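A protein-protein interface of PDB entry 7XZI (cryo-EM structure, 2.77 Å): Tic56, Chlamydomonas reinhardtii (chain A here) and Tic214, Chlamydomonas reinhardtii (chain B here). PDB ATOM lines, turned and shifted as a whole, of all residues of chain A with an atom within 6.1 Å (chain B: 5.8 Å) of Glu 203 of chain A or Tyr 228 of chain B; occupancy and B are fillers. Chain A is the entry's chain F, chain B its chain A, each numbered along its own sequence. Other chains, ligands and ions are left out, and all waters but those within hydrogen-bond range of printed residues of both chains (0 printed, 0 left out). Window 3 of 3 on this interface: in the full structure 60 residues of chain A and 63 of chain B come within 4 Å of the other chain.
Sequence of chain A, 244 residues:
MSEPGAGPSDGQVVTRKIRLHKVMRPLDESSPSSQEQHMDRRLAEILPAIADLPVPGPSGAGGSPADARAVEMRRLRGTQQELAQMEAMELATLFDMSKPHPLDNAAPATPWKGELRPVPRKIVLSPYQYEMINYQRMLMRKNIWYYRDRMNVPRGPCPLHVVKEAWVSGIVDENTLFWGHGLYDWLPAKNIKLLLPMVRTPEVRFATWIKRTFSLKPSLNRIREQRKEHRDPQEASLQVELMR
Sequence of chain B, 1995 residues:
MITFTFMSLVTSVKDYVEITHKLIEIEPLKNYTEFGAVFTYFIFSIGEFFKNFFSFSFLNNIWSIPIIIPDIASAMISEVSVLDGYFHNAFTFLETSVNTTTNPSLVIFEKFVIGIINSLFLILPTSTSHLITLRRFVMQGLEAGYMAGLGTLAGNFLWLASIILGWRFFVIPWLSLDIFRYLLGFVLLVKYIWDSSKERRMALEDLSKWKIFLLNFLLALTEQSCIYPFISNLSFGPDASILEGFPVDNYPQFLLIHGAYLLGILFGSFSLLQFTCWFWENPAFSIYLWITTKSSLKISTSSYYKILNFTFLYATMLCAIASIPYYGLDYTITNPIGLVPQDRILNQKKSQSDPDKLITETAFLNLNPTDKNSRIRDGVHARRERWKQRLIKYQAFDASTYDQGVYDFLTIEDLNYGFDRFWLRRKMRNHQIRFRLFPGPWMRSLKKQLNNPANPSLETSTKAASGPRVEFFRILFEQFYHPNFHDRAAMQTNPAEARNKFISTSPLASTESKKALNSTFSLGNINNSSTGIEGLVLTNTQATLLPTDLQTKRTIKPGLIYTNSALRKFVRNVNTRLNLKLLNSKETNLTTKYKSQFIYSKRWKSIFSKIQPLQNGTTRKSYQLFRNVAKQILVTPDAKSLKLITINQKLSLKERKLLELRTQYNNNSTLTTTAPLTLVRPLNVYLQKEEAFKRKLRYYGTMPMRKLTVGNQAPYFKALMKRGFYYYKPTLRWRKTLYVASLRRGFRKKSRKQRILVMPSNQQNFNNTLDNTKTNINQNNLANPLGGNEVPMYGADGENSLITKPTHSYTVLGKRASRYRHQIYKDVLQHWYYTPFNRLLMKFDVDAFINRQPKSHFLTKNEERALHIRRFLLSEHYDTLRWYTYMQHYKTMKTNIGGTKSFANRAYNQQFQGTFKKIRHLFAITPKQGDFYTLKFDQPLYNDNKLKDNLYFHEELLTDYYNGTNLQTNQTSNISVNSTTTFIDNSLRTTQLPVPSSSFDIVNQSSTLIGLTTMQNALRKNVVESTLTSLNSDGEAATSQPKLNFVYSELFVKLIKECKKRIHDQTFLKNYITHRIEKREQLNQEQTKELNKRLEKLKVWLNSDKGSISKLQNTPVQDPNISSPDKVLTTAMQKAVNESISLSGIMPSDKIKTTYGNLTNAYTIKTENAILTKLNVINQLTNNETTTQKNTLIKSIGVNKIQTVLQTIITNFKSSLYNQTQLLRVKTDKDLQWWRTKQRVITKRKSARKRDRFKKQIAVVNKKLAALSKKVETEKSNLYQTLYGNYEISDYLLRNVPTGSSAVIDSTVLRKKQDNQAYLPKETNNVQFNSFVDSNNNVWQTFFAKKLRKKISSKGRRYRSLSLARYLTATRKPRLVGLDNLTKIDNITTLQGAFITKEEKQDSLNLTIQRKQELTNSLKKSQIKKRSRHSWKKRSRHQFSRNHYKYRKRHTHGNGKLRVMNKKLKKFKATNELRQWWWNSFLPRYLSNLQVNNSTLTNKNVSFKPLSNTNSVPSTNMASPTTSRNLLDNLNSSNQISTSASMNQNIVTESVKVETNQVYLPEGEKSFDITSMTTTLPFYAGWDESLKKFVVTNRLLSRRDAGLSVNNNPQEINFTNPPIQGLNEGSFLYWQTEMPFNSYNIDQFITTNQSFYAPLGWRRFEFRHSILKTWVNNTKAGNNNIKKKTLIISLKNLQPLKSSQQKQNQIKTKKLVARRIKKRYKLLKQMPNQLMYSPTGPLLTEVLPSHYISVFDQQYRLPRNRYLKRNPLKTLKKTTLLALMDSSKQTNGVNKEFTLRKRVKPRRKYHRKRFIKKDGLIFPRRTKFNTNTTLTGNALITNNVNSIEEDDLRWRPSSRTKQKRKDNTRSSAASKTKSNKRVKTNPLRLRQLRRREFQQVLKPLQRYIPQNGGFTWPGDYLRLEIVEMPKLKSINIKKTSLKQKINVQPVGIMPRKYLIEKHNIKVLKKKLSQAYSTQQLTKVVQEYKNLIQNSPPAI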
ATOM      1  N   VAL A 168       0.326 -19.528 -30.461  1.00  0.00           N
ATOM      2  CA  VAL A 168       0.978 -19.383 -29.164  1.00  0.00           C
ATOM      3  C   VAL A 168       0.538 -18.096 -28.479  1.00  0.00           C
ATOM      4  O   VAL A 168       0.281 -18.075 -27.270  1.00  0.00           O
ATOM      5  CB  VAL A 168       2.508 -19.445 -29.330  1.00  0.00           C
ATOM      6  CG1 VAL A 168       3.201 -19.029 -28.044  1.00  0.00           C
ATOM      7  CG2 VAL A 168       2.939 -20.843 -29.734  1.00  0.00           C
ATOM      8  N   THR A 201       3.390 -28.471 -32.175  1.00  0.00           N
ATOM      9  CA  THR A 201       4.644 -29.048 -31.732  1.00  0.00           C
ATOM     10  C   THR A 201       4.723 -28.964 -30.208  1.00  0.00           C
ATOM     11  O   THR A 201       4.029 -28.151 -29.593  1.00  0.00           O
ATOM     12  CB  THR A 201       5.825 -28.322 -32.377  1.00  0.00           C
ATOM     13  OG1 THR A 201       5.796 -26.940 -32.009  1.00  0.00           O
ATOM     14  CG2 THR A 201       5.759 -28.437 -33.893  1.00  0.00           C
ATOM     15  N   PRO A 202       5.546 -29.807 -29.571  1.00  0.00           N
ATOM     16  CA  PRO A 202       5.610 -29.774 -28.097  1.00  0.00           C
ATOM     17  C   PRO A 202       5.960 -28.407 -27.536  1.00  0.00           C
ATOM     18  O   PRO A 202       5.416 -28.004 -26.497  1.00  0.00           O
ATOM     19  CB  PRO A 202       6.692 -30.814 -27.774  1.00  0.00           C
ATOM     20  CG  PRO A 202       6.693 -31.731 -28.938  1.00  0.00           C
ATOM     21  CD  PRO A 202       6.375 -30.889 -30.134  1.00  0.00           C
ATOM     22  N   GLU A 203       6.858 -27.679 -28.202  1.00  0.00           N
ATOM     23  CA  GLU A 203       7.188 -26.328 -27.764  1.00  0.00           C
ATOM     24  C   GLU A 203       5.986 -25.400 -27.869  1.00  0.00           C
ATOM     25  O   GLU A 203       5.763 -24.563 -26.987  1.00  0.00           O
ATOM     26  CB  GLU A 203       8.351 -25.780 -28.586  1.00  0.00           C
ATOM     27  CG  GLU A 203       8.704 -24.348 -28.261  1.00  0.00           C
ATOM     28  CD  GLU A 203       9.758 -23.791 -29.185  1.00  0.00           C
ATOM     29  OE1 GLU A 203       9.626 -23.954 -30.416  1.00  0.00           O
ATOM     30  OE2 GLU A 203      10.725 -23.193 -28.676  1.00  0.00           O
ATOM     31  N   VAL A 204       5.206 -25.529 -28.943  1.00  0.00           N
ATOM     32  CA  VAL A 204       4.004 -24.714 -29.089  1.00  0.00           C
ATOM     33  C   VAL A 204       3.020 -25.020 -27.969  1.00  0.00           C
ATOM     34  O   VAL A 204       2.411 -24.110 -27.395  1.00  0.00           O
ATOM     35  CB  VAL A 204       3.372 -24.930 -30.477  1.00  0.00           C
ATOM     36  CG1 VAL A 204       1.947 -24.410 -30.498  1.00  0.00           C
ATOM     37  CG2 VAL A 204       4.199 -24.234 -31.541  1.00  0.00           C
ATOM     38  N   ARG A 205       2.850 -26.301 -27.640  1.00  0.00           N
ATOM     39  CA  ARG A 205       1.955 -26.670 -26.547  1.00  0.00           C
ATOM     40  C   ARG A 205       2.423 -26.080 -25.222  1.00  0.00           C
ATOM     41  O   ARG A 205       1.624 -25.501 -24.476  1.00  0.00           O
ATOM     42  CB  ARG A 205       1.853 -28.191 -26.448  1.00  0.00           C
ATOM     43  CG  ARG A 205       1.116 -28.833 -27.609  1.00  0.00           C
ATOM     44  CD  ARG A 205       1.087 -30.346 -27.487  1.00  0.00           C
ATOM     45  NE  ARG A 205       2.296 -30.967 -28.009  1.00  0.00           N
ATOM     46  CZ  ARG A 205       2.520 -32.277 -28.017  1.00  0.00           C
ATOM     47  NH1 ARG A 205       1.641 -33.132 -27.521  1.00  0.00           N
ATOM     48  NH2 ARG A 205       3.652 -32.739 -28.538  1.00  0.00           N
ATOM     49  N   PHE A 206       3.715 -26.208 -24.918  1.00  0.00           N
ATOM     50  CA  PHE A 206       4.229 -25.685 -23.657  1.00  0.00           C
ATOM     51  C   PHE A 206       4.083 -24.168 -23.587  1.00  0.00           C
ATOM     52  O   PHE A 206       3.650 -23.620 -22.562  1.00  0.00           O
ATOM     53  CB  PHE A 206       5.687 -26.110 -23.488  1.00  0.00           C
ATOM     54  CG  PHE A 206       6.293 -25.720 -22.174  1.00  0.00           C
ATOM     55  CD1 PHE A 206       5.873 -26.314 -20.996  1.00  0.00           C
ATOM     56  CD2 PHE A 206       7.303 -24.775 -22.120  1.00  0.00           C
ATOM     57  CE1 PHE A 206       6.436 -25.960 -19.788  1.00  0.00           C
ATOM     58  CE2 PHE A 206       7.872 -24.419 -20.915  1.00  0.00           C
ATOM     59  CZ  PHE A 206       7.437 -25.010 -19.747  1.00  0.00           C
ATOM     60  N   ALA A 207       4.410 -23.474 -24.679  1.00  0.00           N
ATOM     61  CA  ALA A 207       4.318 -22.020 -24.696  1.00  0.00           C
ATOM     62  C   ALA A 207       2.877 -21.540 -24.602  1.00  0.00           C
ATOM     63  O   ALA A 207       2.599 -20.565 -23.897  1.00  0.00           O
ATOM     64  CB  ALA A 207       4.986 -21.468 -25.953  1.00  0.00           C
ATOM     65  N   THR A 208       1.942 -22.201 -25.293  1.00  0.00           N
ATOM     66  CA  THR A 208       0.550 -21.776 -25.206  1.00  0.00           C
ATOM     67  C   THR A 208      -0.029 -22.078 -23.829  1.00  0.00           C
ATOM     68  O   THR A 208      -0.853 -21.312 -23.321  1.00  0.00           O
ATOM     69  CB  THR A 208      -0.290 -22.416 -26.319  1.00  0.00           C
ATOM     70  OG1 THR A 208      -1.561 -21.757 -26.392  1.00  0.00           O
ATOM     71  CG2 THR A 208      -0.521 -23.896 -26.075  1.00  0.00           C
ATOM     72  N   THR B 126      19.446 -18.215 -26.488  1.00  0.00           N
ATOM     73  CA  THR B 126      18.898 -18.890 -27.656  1.00  0.00           C
ATOM     74  C   THR B 126      19.312 -18.268 -28.984  1.00  0.00           C
ATOM     75  O   THR B 126      18.821 -18.710 -30.028  1.00  0.00           O
ATOM     76  CB  THR B 126      17.361 -18.922 -27.589  1.00  0.00           C
ATOM     77  OG1 THR B 126      16.858 -17.594 -27.404  1.00  0.00           O
ATOM     78  CG2 THR B 126      16.884 -19.808 -26.448  1.00  0.00           C
ATOM     79  N   CYS B 226      17.657 -17.725 -34.605  1.00  0.00           N
ATOM     80  CA  CYS B 226      17.145 -17.890 -33.250  1.00  0.00           C
ATOM     81  C   CYS B 226      16.631 -19.311 -33.091  1.00  0.00           C
ATOM     82  O   CYS B 226      15.893 -19.804 -33.948  1.00  0.00           O
ATOM     83  CB  CYS B 226      16.032 -16.879 -32.953  1.00  0.00           C
ATOM     84  SG  CYS B 226      15.207 -17.103 -31.357  1.00  0.00           S
ATOM     85  N   ILE B 227      17.030 -19.962 -32.007  1.00  0.00           N
ATOM     86  CA  ILE B 227      16.500 -21.261 -31.641  1.00  0.00           C
ATOM     87  C   ILE B 227      15.452 -21.045 -30.559  1.00  0.00           C
ATOM     88  O   ILE B 227      15.421 -20.013 -29.883  1.00  0.00           O
ATOM     89  CB  ILE B 227      17.612 -22.230 -31.169  1.00  0.00           C
ATOM     90  CG1 ILE B 227      17.145 -23.686 -31.259  1.00  0.00           C
ATOM     91  CG2 ILE B 227      18.053 -21.898 -29.752  1.00  0.00           C
ATOM     92  CD1 ILE B 227      18.182 -24.688 -30.796  1.00  0.00           C
ATOM     93  N   TYR B 228      14.569 -22.024 -30.402  1.00  0.00           N
ATOM     94  CA  TYR B 228      13.466 -21.956 -29.449  1.00  0.00           C
ATOM     95  C   TYR B 228      12.607 -20.699 -29.615  1.00  0.00           C
ATOM     96  O   TYR B 228      12.572 -19.844 -28.725  1.00  0.00           O
ATOM     97  CB  TYR B 228      13.986 -22.062 -28.022  1.00  0.00           C
ATOM     98  CG  TYR B 228      14.234 -23.479 -27.562  1.00  0.00           C
ATOM     99  CD1 TYR B 228      13.184 -24.282 -27.142  1.00  0.00           C
ATOM    100  CD2 TYR B 228      15.514 -24.012 -27.543  1.00  0.00           C
ATOM    101  CE1 TYR B 228      13.398 -25.574 -26.722  1.00  0.00           C
ATOM    102  CE2 TYR B 228      15.740 -25.307 -27.121  1.00  0.00           C
ATOM    103  CZ  TYR B 228      14.677 -26.083 -26.711  1.00  0.00           C
ATOM    104  OH  TYR B 228      14.888 -27.374 -26.289  1.00  0.00           O
ATOM    105  N   PRO B 229      11.901 -20.553 -30.746  1.00  0.00           N
ATOM    106  CA  PRO B 229      10.930 -19.456 -30.855  1.00  0.00           C
ATOM    107  C   PRO B 229       9.675 -19.742 -30.047  1.00  0.00           C
ATOM    108  O   PRO B 229       9.552 -20.816 -29.451  1.00  0.00           O
ATOM    109  CB  PRO B 229      10.631 -19.392 -32.360  1.00  0.00           C
ATOM    110  CG  PRO B 229      11.726 -20.181 -33.017  1.00  0.00           C
ATOM    111  CD  PRO B 229      12.069 -21.246 -32.033  1.00  0.00           C
ATOM    112  N   PHE B 230       8.763 -18.767 -29.985  1.00  0.00           N
ATOM    113  CA  PHE B 230       7.475 -18.891 -29.303  1.00  0.00           C
ATOM    114  C   PHE B 230       7.676 -18.895 -27.791  1.00  0.00           C
ATOM    115  O   PHE B 230       6.707 -18.885 -27.026  1.00  0.00           O
ATOM    116  CB  PHE B 230       6.720 -20.145 -29.764  1.00  0.00           C
ATOM    117  CG  PHE B 230       6.799 -20.388 -31.245  1.00  0.00           C
ATOM    118  CD1 PHE B 230       6.580 -19.357 -32.141  1.00  0.00           C
ATOM    119  CD2 PHE B 230       7.114 -21.643 -31.740  1.00  0.00           C
ATOM    120  CE1 PHE B 230       6.664 -19.574 -33.504  1.00  0.00           C
ATOM    121  CE2 PHE B 230       7.196 -21.865 -33.100  1.00  0.00           C
ATOM    122  CZ  PHE B 230       6.971 -20.829 -33.984  1.00  0.00           C
ATOM    123  N   ILE B 231       8.935 -18.900 -27.356  1.00  0.00           N
ATOM    124  CA  ILE B 231       9.273 -18.751 -25.954  1.00  0.00           C
ATOM    125  C   ILE B 231      10.069 -17.477 -25.686  1.00  0.00           C
ATOM    126  O   ILE B 231       9.838 -16.821 -24.664  1.00  0.00           O
ATOM    127  CB  ILE B 231      10.035 -19.990 -25.443  1.00  0.00           C
ATOM    128  CG1 ILE B 231       9.171 -21.240 -25.611  1.00  0.00           C
ATOM    129  CG2 ILE B 231      10.439 -19.818 -23.987  1.00  0.00           C
ATOM    130  CD1 ILE B 231       9.846 -22.510 -25.165  1.00  0.00           C
ATOM    131  N   SER B 232      10.984 -17.099 -26.577  1.00  0.00           N
ATOM    132  CA  SER B 232      11.646 -15.806 -26.479  1.00  0.00           C
ATOM    133  C   SER B 232      10.746 -14.659 -26.910  1.00  0.00           C
ATOM    134  O   SER B 232      11.114 -13.495 -26.716  1.00  0.00           O
ATOM    135  CB  SER B 232      12.925 -15.799 -27.320  1.00  0.00           C
ATOM    136  OG  SER B 232      13.778 -16.872 -26.963  1.00  0.00           O
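O of Phe 230 of chain B touches CG1 of Val 168 of chain A, 3.7 Å away.
OE2 of Glu 203 of chain A touches CD1 of Tyr 228 of chain B, 3.1 Å away.
Glu 203 of chain A touches Phe 230 of chain B (OE1 to CD2, 3.7 Å).
Glu 203 of chain A touches Ile 231 of chain B.
CG2 of Val 204 of chain A touches CD2 of Phe 230 of chain B (3.9 Å).
Ala 207 of chain A touches Phe 230 of chain B (CB to O, 3.3 Å).
Of the printed residues of chain B, Val 168 of chain A touches Phe 230.
Pro 202 of chain A touches none of the printed residues of chain B.
Printed residues of chain B within 4 Å of Val 204 of chain A: Phe 230 (3.9 Å).
Ile 227 of chain B touches none of the printed residues of chain A.
Of the printed residues of chain A, Pro 229 of chain B touches Glu 203 (2.8 Å).
Of the printed residues of chain A, Phe 230 of chain B touches Val 168 (3.7 Å), Glu 203 (3.7 Å), Val 204 (3.9 Å) and Ala 207 (3.3 Å).
Of the printed residues of chain A, Ile 231 of chain B touches Glu 203.
The nearest residue of chain B that does not touch Glu 203 of chain A is Ile 227 of chain B (5.5 Å).
The backbone carbonyl oxygen of Pro 229 of chain B sits close to the side-chain carboxylate of Glu 203 of chain A.
The side-chain hydroxyl (OG1) of Thr 201 of chain A sits close to the backbone NH (N) of Val 204 of chain A, 3.4 Å away.
Hydrophobic or aromatic side chains of chain A that line the printed part of chain B: Val 168, Val 204 and Ala 207.
Of the 8 printed residues of chain B, 4 touch a printed residue of chain A.
Hydrophobic or aromatic side chains of chain B within 4 Å of the printed part of chain A: Tyr 228, Pro 229, Phe 230 and Ile 231.
Among the printed residues, no Asp or Glu carboxylate lies within 4 Å of a Lys or Arg side-chain nitrogen of the other chain.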
